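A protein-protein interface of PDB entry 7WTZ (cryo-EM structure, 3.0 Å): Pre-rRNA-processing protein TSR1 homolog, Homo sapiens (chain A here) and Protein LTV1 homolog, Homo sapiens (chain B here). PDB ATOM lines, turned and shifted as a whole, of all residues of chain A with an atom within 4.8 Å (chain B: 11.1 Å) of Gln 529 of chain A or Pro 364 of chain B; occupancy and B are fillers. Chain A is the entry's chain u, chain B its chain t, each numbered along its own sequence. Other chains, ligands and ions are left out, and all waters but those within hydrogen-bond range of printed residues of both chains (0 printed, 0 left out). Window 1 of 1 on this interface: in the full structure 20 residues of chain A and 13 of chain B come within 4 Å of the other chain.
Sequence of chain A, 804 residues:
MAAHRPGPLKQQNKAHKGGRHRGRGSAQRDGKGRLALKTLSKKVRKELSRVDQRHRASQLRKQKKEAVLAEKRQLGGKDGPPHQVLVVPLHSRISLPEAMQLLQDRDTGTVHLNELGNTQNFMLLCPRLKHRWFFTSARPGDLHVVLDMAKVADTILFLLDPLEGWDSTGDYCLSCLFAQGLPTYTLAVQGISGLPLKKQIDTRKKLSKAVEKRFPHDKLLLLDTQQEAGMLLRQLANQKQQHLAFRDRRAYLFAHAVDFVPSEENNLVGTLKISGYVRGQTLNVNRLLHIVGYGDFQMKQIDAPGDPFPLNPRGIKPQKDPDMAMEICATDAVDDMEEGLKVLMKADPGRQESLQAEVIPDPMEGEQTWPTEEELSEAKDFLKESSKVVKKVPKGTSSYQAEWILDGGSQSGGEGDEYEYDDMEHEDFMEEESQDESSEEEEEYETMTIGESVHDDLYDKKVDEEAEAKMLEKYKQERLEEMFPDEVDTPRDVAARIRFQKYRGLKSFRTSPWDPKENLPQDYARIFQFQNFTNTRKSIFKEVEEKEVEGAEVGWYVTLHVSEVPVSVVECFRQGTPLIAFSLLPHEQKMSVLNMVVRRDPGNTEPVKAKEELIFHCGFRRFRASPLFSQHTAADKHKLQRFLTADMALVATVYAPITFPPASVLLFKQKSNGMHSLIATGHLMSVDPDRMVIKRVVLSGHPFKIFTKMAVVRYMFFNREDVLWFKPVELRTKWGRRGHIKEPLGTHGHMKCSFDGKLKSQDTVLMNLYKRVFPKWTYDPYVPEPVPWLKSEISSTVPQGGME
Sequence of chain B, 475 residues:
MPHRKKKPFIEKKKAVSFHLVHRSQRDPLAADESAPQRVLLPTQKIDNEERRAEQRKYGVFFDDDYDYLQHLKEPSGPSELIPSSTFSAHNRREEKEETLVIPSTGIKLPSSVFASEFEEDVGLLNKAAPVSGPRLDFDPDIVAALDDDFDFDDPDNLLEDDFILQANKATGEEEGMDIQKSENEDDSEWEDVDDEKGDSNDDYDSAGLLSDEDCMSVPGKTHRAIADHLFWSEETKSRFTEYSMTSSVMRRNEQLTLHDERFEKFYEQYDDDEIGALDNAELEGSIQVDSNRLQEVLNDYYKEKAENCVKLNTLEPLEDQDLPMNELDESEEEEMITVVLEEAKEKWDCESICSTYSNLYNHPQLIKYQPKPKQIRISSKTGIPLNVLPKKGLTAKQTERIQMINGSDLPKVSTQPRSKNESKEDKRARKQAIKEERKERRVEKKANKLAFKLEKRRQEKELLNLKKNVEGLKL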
ATOM      1  N   LYS A 517     -14.835  23.172  17.064  1.00  0.00           N
ATOM      2  CA  LYS A 517     -14.522  24.492  17.595  1.00  0.00           C
ATOM      3  C   LYS A 517     -15.269  25.596  16.853  1.00  0.00           C
ATOM      4  O   LYS A 517     -14.798  26.732  16.786  1.00  0.00           O
ATOM      5  CB  LYS A 517     -13.015  24.736  17.541  1.00  0.00           C
ATOM      6  CG  LYS A 517     -12.219  23.809  18.441  1.00  0.00           C
ATOM      7  CD  LYS A 517     -10.728  24.023  18.301  1.00  0.00           C
ATOM      8  CE  LYS A 517      -9.972  23.144  19.275  1.00  0.00           C
ATOM      9  NZ  LYS A 517     -10.166  21.704  18.960  1.00  0.00           N
ATOM     10  N   LEU A 520     -18.109  28.494  19.984  1.00  0.00           N
ATOM     11  CA  LEU A 520     -17.884  28.124  21.366  1.00  0.00           C
ATOM     12  C   LEU A 520     -18.397  29.211  22.304  1.00  0.00           C
ATOM     13  O   LEU A 520     -18.305  30.401  21.991  1.00  0.00           O
ATOM     14  CB  LEU A 520     -16.392  27.889  21.633  1.00  0.00           C
ATOM     15  CG  LEU A 520     -15.795  26.633  21.000  1.00  0.00           C
ATOM     16  CD1 LEU A 520     -14.348  26.452  21.424  1.00  0.00           C
ATOM     17  CD2 LEU A 520     -16.620  25.400  21.319  1.00  0.00           C
ATOM     18  N   TYR A 524     -16.200  28.345  27.625  1.00  0.00           N
ATOM     19  CA  TYR A 524     -15.054  27.560  27.176  1.00  0.00           C
ATOM     20  C   TYR A 524     -13.764  28.365  27.202  1.00  0.00           C
ATOM     21  O   TYR A 524     -12.677  27.780  27.214  1.00  0.00           O
ATOM     22  CB  TYR A 524     -15.290  26.996  25.777  1.00  0.00           C
ATOM     23  CG  TYR A 524     -15.947  25.637  25.766  1.00  0.00           C
ATOM     24  CD1 TYR A 524     -16.765  25.225  26.807  1.00  0.00           C
ATOM     25  CD2 TYR A 524     -15.736  24.759  24.715  1.00  0.00           C
ATOM     26  CE1 TYR A 524     -17.358  23.980  26.796  1.00  0.00           C
ATOM     27  CE2 TYR A 524     -16.321  23.515  24.695  1.00  0.00           C
ATOM     28  CZ  TYR A 524     -17.133  23.131  25.736  1.00  0.00           C
ATOM     29  OH  TYR A 524     -17.719  21.889  25.716  1.00  0.00           O
ATOM     30  N   ILE A 527     -11.990  27.389  30.756  1.00  0.00           N
ATOM     31  CA  ILE A 527     -11.628  26.025  31.133  1.00  0.00           C
ATOM     32  C   ILE A 527     -10.341  25.616  30.430  1.00  0.00           C
ATOM     33  O   ILE A 527      -9.844  26.329  29.554  1.00  0.00           O
ATOM     34  CB  ILE A 527     -12.757  25.034  30.802  1.00  0.00           C
ATOM     35  CG1 ILE A 527     -12.993  24.982  29.295  1.00  0.00           C
ATOM     36  CG2 ILE A 527     -14.030  25.412  31.519  1.00  0.00           C
ATOM     37  CD1 ILE A 527     -13.839  23.819  28.862  1.00  0.00           C
ATOM     38  N   PHE A 528      -9.811  24.451  30.791  1.00  0.00           N
ATOM     39  CA  PHE A 528      -8.547  23.955  30.264  1.00  0.00           C
ATOM     40  C   PHE A 528      -8.804  22.739  29.388  1.00  0.00           C
ATOM     41  O   PHE A 528      -9.753  21.988  29.626  1.00  0.00           O
ATOM     42  CB  PHE A 528      -7.584  23.588  31.395  1.00  0.00           C
ATOM     43  CG  PHE A 528      -7.000  24.774  32.099  1.00  0.00           C
ATOM     44  CD1 PHE A 528      -7.693  25.398  33.121  1.00  0.00           C
ATOM     45  CD2 PHE A 528      -5.755  25.261  31.744  1.00  0.00           C
ATOM     46  CE1 PHE A 528      -7.159  26.489  33.773  1.00  0.00           C
ATOM     47  CE2 PHE A 528      -5.214  26.352  32.392  1.00  0.00           C
ATOM     48  CZ  PHE A 528      -5.918  26.968  33.408  1.00  0.00           C
ATOM     49  N   GLN A 529      -7.971  22.552  28.374  1.00  0.00           N
ATOM     50  CA  GLN A 529      -8.060  21.392  27.503  1.00  0.00           C
ATOM     51  C   GLN A 529      -6.764  20.590  27.572  1.00  0.00           C
ATOM     52  O   GLN A 529      -5.744  21.049  28.089  1.00  0.00           O
ATOM     53  CB  GLN A 529      -8.359  21.821  26.064  1.00  0.00           C
ATOM     54  CG  GLN A 529      -9.166  20.806  25.265  1.00  0.00           C
ATOM     55  CD  GLN A 529      -9.301  21.180  23.806  1.00  0.00           C
ATOM     56  OE1 GLN A 529      -9.716  22.287  23.473  1.00  0.00           O
ATOM     57  NE2 GLN A 529      -8.957  20.250  22.925  1.00  0.00           N
ATOM     58  N   PHE A 530      -6.816  19.370  27.052  1.00  0.00           N
ATOM     59  CA  PHE A 530      -5.653  18.499  26.977  1.00  0.00           C
ATOM     60  C   PHE A 530      -5.276  18.305  25.517  1.00  0.00           C
ATOM     61  O   PHE A 530      -6.138  18.005  24.684  1.00  0.00           O
ATOM     62  CB  PHE A 530      -5.935  17.146  27.632  1.00  0.00           C
ATOM     63  CG  PHE A 530      -5.543  17.084  29.076  1.00  0.00           C
ATOM     64  CD1 PHE A 530      -6.115  17.943  29.991  1.00  0.00           C
ATOM     65  CD2 PHE A 530      -4.591  16.184  29.515  1.00  0.00           C
ATOM     66  CE1 PHE A 530      -5.756  17.893  31.317  1.00  0.00           C
ATOM     67  CE2 PHE A 530      -4.232  16.132  30.845  1.00  0.00           C
ATOM     68  CZ  PHE A 530      -4.815  16.989  31.746  1.00  0.00           C
ATOM     69  N   GLN A 531      -3.992  18.501  25.206  1.00  0.00           N
ATOM     70  CA  GLN A 531      -3.512  18.256  23.850  1.00  0.00           C
ATOM     71  C   GLN A 531      -3.630  16.781  23.493  1.00  0.00           C
ATOM     72  O   GLN A 531      -4.005  16.427  22.370  1.00  0.00           O
ATOM     73  CB  GLN A 531      -2.069  18.736  23.711  1.00  0.00           C
ATOM     74  CG  GLN A 531      -1.592  18.844  22.277  1.00  0.00           C
ATOM     75  CD  GLN A 531      -0.089  18.967  22.172  1.00  0.00           C
ATOM     76  OE1 GLN A 531       0.652  18.182  22.762  1.00  0.00           O
ATOM     77  NE2 GLN A 531       0.371  19.960  21.423  1.00  0.00           N
ATOM     78  N   PRO A 689     -13.604  18.798  26.435  1.00  0.00           N
ATOM     79  CA  PRO A 689     -14.694  19.694  26.035  1.00  0.00           C
ATOM     80  C   PRO A 689     -15.032  19.638  24.556  1.00  0.00           C
ATOM     81  O   PRO A 689     -15.975  20.320  24.132  1.00  0.00           O
ATOM     82  CB  PRO A 689     -14.159  21.077  26.418  1.00  0.00           C
ATOM     83  CG  PRO A 689     -12.693  20.936  26.349  1.00  0.00           C
ATOM     84  CD  PRO A 689     -12.388  19.542  26.806  1.00  0.00           C
ATOM     85  N   ASP A 690     -14.300  18.858  23.761  1.00  0.00           N
ATOM     86  CA  ASP A 690     -14.582  18.767  22.335  1.00  0.00           C
ATOM     87  C   ASP A 690     -15.587  17.677  22.003  1.00  0.00           C
ATOM     88  O   ASP A 690     -15.866  17.451  20.821  1.00  0.00           O
ATOM     89  CB  ASP A 690     -13.288  18.531  21.555  1.00  0.00           C
ATOM     90  CG  ASP A 690     -12.631  19.825  21.110  1.00  0.00           C
ATOM     91  OD1 ASP A 690     -13.035  20.899  21.606  1.00  0.00           O
ATOM     92  OD2 ASP A 690     -11.713  19.768  20.265  1.00  0.00           O
ATOM     93  N   LEU B 360     -13.843  31.243  14.153  1.00  0.00           N
ATOM     94  CA  LEU B 360     -13.079  30.484  15.146  1.00  0.00           C
ATOM     95  C   LEU B 360     -12.625  31.449  16.240  1.00  0.00           C
ATOM     96  O   LEU B 360     -11.809  32.349  16.025  1.00  0.00           O
ATOM     97  CB  LEU B 360     -11.898  29.784  14.482  1.00  0.00           C
ATOM     98  CG  LEU B 360     -12.027  28.393  13.841  1.00  0.00           C
ATOM     99  CD1 LEU B 360     -12.230  27.328  14.894  1.00  0.00           C
ATOM    100  CD2 LEU B 360     -13.131  28.319  12.791  1.00  0.00           C
ATOM    101  N   TYR B 361     -13.162  31.247  17.443  1.00  0.00           N
ATOM    102  CA  TYR B 361     -12.988  32.189  18.540  1.00  0.00           C
ATOM    103  C   TYR B 361     -12.957  31.446  19.872  1.00  0.00           C
ATOM    104  O   TYR B 361     -13.334  30.273  19.939  1.00  0.00           O
ATOM    105  CB  TYR B 361     -14.119  33.227  18.529  1.00  0.00           C
ATOM    106  CG  TYR B 361     -13.841  34.477  19.326  1.00  0.00           C
ATOM    107  CD1 TYR B 361     -12.779  35.309  18.997  1.00  0.00           C
ATOM    108  CD2 TYR B 361     -14.647  34.835  20.398  1.00  0.00           C
ATOM    109  CE1 TYR B 361     -12.521  36.458  19.719  1.00  0.00           C
ATOM    110  CE2 TYR B 361     -14.399  35.983  21.127  1.00  0.00           C
ATOM    111  CZ  TYR B 361     -13.334  36.790  20.784  1.00  0.00           C
ATOM    112  OH  TYR B 361     -13.083  37.933  21.507  1.00  0.00           O
ATOM    113  N   ASN B 362     -12.439  32.133  20.903  1.00  0.00           N
ATOM    114  CA  ASN B 362     -12.393  31.803  22.338  1.00  0.00           C
ATOM    115  C   ASN B 362     -12.246  30.318  22.680  1.00  0.00           C
ATOM    116  O   ASN B 362     -13.057  29.749  23.419  1.00  0.00           O
ATOM    117  CB  ASN B 362     -13.583  32.446  23.096  1.00  0.00           C
ATOM    118  CG  ASN B 362     -14.968  31.940  22.677  1.00  0.00           C
ATOM    119  OD1 ASN B 362     -15.122  31.008  21.901  1.00  0.00           O
ATOM    120  ND2 ASN B 362     -15.995  32.585  23.221  1.00  0.00           N
ATOM    121  N   HIS B 363     -11.185  29.700  22.183  1.00  0.00           N
ATOM    122  CA  HIS B 363     -10.846  28.312  22.447  1.00  0.00           C
ATOM    123  C   HIS B 363     -10.305  28.174  23.860  1.00  0.00           C
ATOM    124  O   HIS B 363      -9.705  29.111  24.397  1.00  0.00           O
ATOM    125  CB  HIS B 363      -9.800  27.806  21.444  1.00  0.00           C
ATOM    126  CG  HIS B 363     -10.190  28.008  20.015  1.00  0.00           C
ATOM    127  ND1 HIS B 363      -9.618  28.977  19.219  1.00  0.00           N
ATOM    128  CD2 HIS B 363     -11.104  27.378  19.243  1.00  0.00           C
ATOM    129  CE1 HIS B 363     -10.158  28.928  18.015  1.00  0.00           C
ATOM    130  NE2 HIS B 363     -11.063  27.966  18.003  1.00  0.00           N
ATOM    131  N   PRO B 364     -10.515  27.021  24.498  1.00  0.00           N
ATOM    132  CA  PRO B 364      -9.906  26.789  25.813  1.00  0.00           C
ATOM    133  C   PRO B 364      -8.396  26.650  25.716  1.00  0.00           C
ATOM    134  O   PRO B 364      -7.856  26.223  24.693  1.00  0.00           O
ATOM    135  CB  PRO B 364     -10.556  25.483  26.282  1.00  0.00           C
ATOM    136  CG  PRO B 364     -11.077  24.845  25.052  1.00  0.00           C
ATOM    137  CD  PRO B 364     -11.466  25.957  24.139  1.00  0.00           C
ATOM    138  N   GLN B 365      -7.717  27.016  26.799  1.00  0.00           N
ATOM    139  CA  GLN B 365      -6.267  26.887  26.862  1.00  0.00           C
ATOM    140  C   GLN B 365      -5.893  25.420  27.024  1.00  0.00           C
ATOM    141  O   GLN B 365      -6.262  24.786  28.017  1.00  0.00           O
ATOM    142  CB  GLN B 365      -5.714  27.715  28.018  1.00  0.00           C
ATOM    143  CG  GLN B 365      -4.273  27.413  28.375  1.00  0.00           C
ATOM    144  CD  GLN B 365      -3.737  28.341  29.446  1.00  0.00           C
ATOM    145  OE1 GLN B 365      -4.318  29.389  29.723  1.00  0.00           O
ATOM    146  NE2 GLN B 365      -2.624  27.956  30.059  1.00  0.00           N
ATOM    147  N   LEU B 366      -5.162  24.882  26.058  1.00  0.00           N
ATOM    148  CA  LEU B 366      -4.833  23.465  26.042  1.00  0.00           C
ATOM    149  C   LEU B 366      -3.524  23.218  26.779  1.00  0.00           C
ATOM    150  O   LEU B 366      -2.604  24.038  26.731  1.00  0.00           O
ATOM    151  CB  LEU B 366      -4.748  22.919  24.611  1.00  0.00           C
ATOM    152  CG  LEU B 366      -3.588  23.241  23.666  1.00  0.00           C
ATOM    153  CD1 LEU B 366      -3.596  22.252  22.518  1.00  0.00           C
ATOM    154  CD2 LEU B 366      -3.676  24.659  23.122  1.00  0.00           C
ATOM    155  N   ILE B 367      -3.461  22.087  27.475  1.00  0.00           N
ATOM    156  CA  ILE B 367      -2.278  21.707  28.237  1.00  0.00           C
ATOM    157  C   ILE B 367      -1.407  20.815  27.362  1.00  0.00           C
ATOM    158  O   ILE B 367      -1.854  19.763  26.892  1.00  0.00           O
ATOM    159  CB  ILE B 367      -2.669  21.003  29.541  1.00  0.00           C
ATOM    160  CG1 ILE B 367      -3.496  21.948  30.416  1.00  0.00           C
ATOM    161  CG2 ILE B 367      -1.435  20.523  30.280  1.00  0.00           C
ATOM    162  CD1 ILE B 367      -4.388  21.245  31.404  1.00  0.00           C
ATOM    163  N   LYS B 368      -0.163  21.230  27.149  1.00  0.00           N
ATOM    164  CA  LYS B 368       0.717  20.586  26.187  1.00  0.00           C
ATOM    165  C   LYS B 368       1.251  19.264  26.721  1.00  0.00           C
ATOM    166  O   LYS B 368       1.268  19.017  27.930  1.00  0.00           O
ATOM    167  CB  LYS B 368       1.886  21.504  25.832  1.00  0.00           C
ATOM    168  CG  LYS B 368       1.467  22.832  25.227  1.00  0.00           C
ATOM    169  CD  LYS B 368       0.796  22.638  23.879  1.00  0.00           C
ATOM    170  CE  LYS B 368       0.593  23.968  23.177  1.00  0.00           C
ATOM    171  NZ  LYS B 368      -0.364  24.836  23.915  1.00  0.00           N
ATOM    172  N   TYR B 369       1.687  18.413  25.798  1.00  0.00           N
ATOM    173  CA  TYR B 369       2.314  17.145  26.146  1.00  0.00           C
ATOM    174  C   TYR B 369       3.698  17.049  25.517  1.00  0.00           C
ATOM    175  O   TYR B 369       3.828  16.910  24.301  1.00  0.00           O
ATOM    176  CB  TYR B 369       1.445  15.969  25.696  1.00  0.00           C
ATOM    177  CG  TYR B 369       2.164  14.641  25.732  1.00  0.00           C
ATOM    178  CD1 TYR B 369       2.650  14.122  26.927  1.00  0.00           C
ATOM    179  CD2 TYR B 369       2.361  13.905  24.570  1.00  0.00           C
ATOM    180  CE1 TYR B 369       3.312  12.909  26.964  1.00  0.00           C
ATOM    181  CE2 TYR B 369       3.021  12.691  24.597  1.00  0.00           C
ATOM    182  CZ  TYR B 369       3.494  12.198  25.796  1.00  0.00           C
ATOM    183  OH  TYR B 369       4.150  10.990  25.828  1.00  0.00           O
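Of the printed residues of chain B, Tyr 524 of chain A touches Pro 364 (3.3 Å).
Of chain B, only Gln 365 and Ile 367 come within 4 Å of Phe 528 of chain A.
Of chain B, only Pro 364, Gln 365, Leu 366 and Ile 367 come within 4 Å of Gln 529 of chain A.
Of chain B, only Ile 367 (3.6 Å) comes within 4 Å of Phe 530 of chain A.
Asp 690 of chain A touches none of the printed residues of chain B.
Printed residues of chain A within 4 Å of Leu 360 of chain B: Lys 517 (3.2 Å).
Of the printed residues of chain A, Pro 364 of chain B touches Leu 520 (3.99 Å), Tyr 524 (3.3 Å), Ile 527 (3.5 Å) and Gln 529 (3.3 Å).
The nearest printed residue of chain A that does not touch Asn 362 of chain B is Tyr 524 of chain A (4.1 Å).
The side-chain amino group (NZ) of Lys 517 of chain A lies within salt-bridge range of the side-chain carboxylate (OD2) of Asp 690 of chain A (2.8 Å).
The side-chain hydroxyl of Tyr 524 of chain A sits at hydrogen-bond distance from the backbone carbonyl oxygen of Pro 689 of chain A, 2.8 Å away.
CD of Lys 517 of chain A touches CD2 of His 363 of chain B, 3.5 Å away.
Pro 364 of chain B touches Leu 520 of chain A (CD to CD1, 3.99 Å).
CA of Pro 364 of chain B touches O of Tyr 524 of chain A, at 3.3 Å.
CB of Pro 364 of chain B touches O of Ile 527 of chain A (3.5 Å).
Gln 365 of chain B touches Ile 527 of chain A (N to O, 3.5 Å).
Phe 528 of chain A touches Gln 365 of chain B (CA to O, 3.3 Å).
Ile 367 of chain B touches Phe 528 of chain A (CD1 to CB, 3.96 Å).
Pro 364 of chain B touches Gln 529 of chain A (CG to OE1, 3.3 Å).
Gln 529 of chain A touches Leu 366 of chain B.
CD1 of Leu 366 of chain B touches CG of Gln 531 of chain A (3.96 Å).
Hydrophobic or aromatic side chains of chain B within 4 Å of the printed part of chain A: Leu 360, His 363, Pro 364, Leu 366, Ile 367 and Tyr 369.
Among the printed residues, 18 pairs touch across the chains.
Among the printed residues, no Asp or Glu carboxylate lies within 4 Å of a Lys or Arg side-chain nitrogen of the other chain.
OD1 of Asn 362 of chain B sits close to O of Leu 520 of chain A (3.2 Å).
The backbone NH (N) of Gln 529 of chain A lies within hydrogen-bond range of the backbone carbonyl oxygen (O) of Gln 365 of chain B (2.8 Å).
O of Gln 529 of chain A sits at hydrogen-bond distance from N of Ile 367 of chain B (2.6 Å).
The backbone carbonyl oxygen of Ile 367 of chain B lies within hydrogen-bond range of the backbone NH of Gln 531 of chain A (3.0 Å).
The backbone NH of Tyr 369 of chain B lies within hydrogen-bond range of the side-chain amide oxygen of Gln 531 of chain A (3.2 Å).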
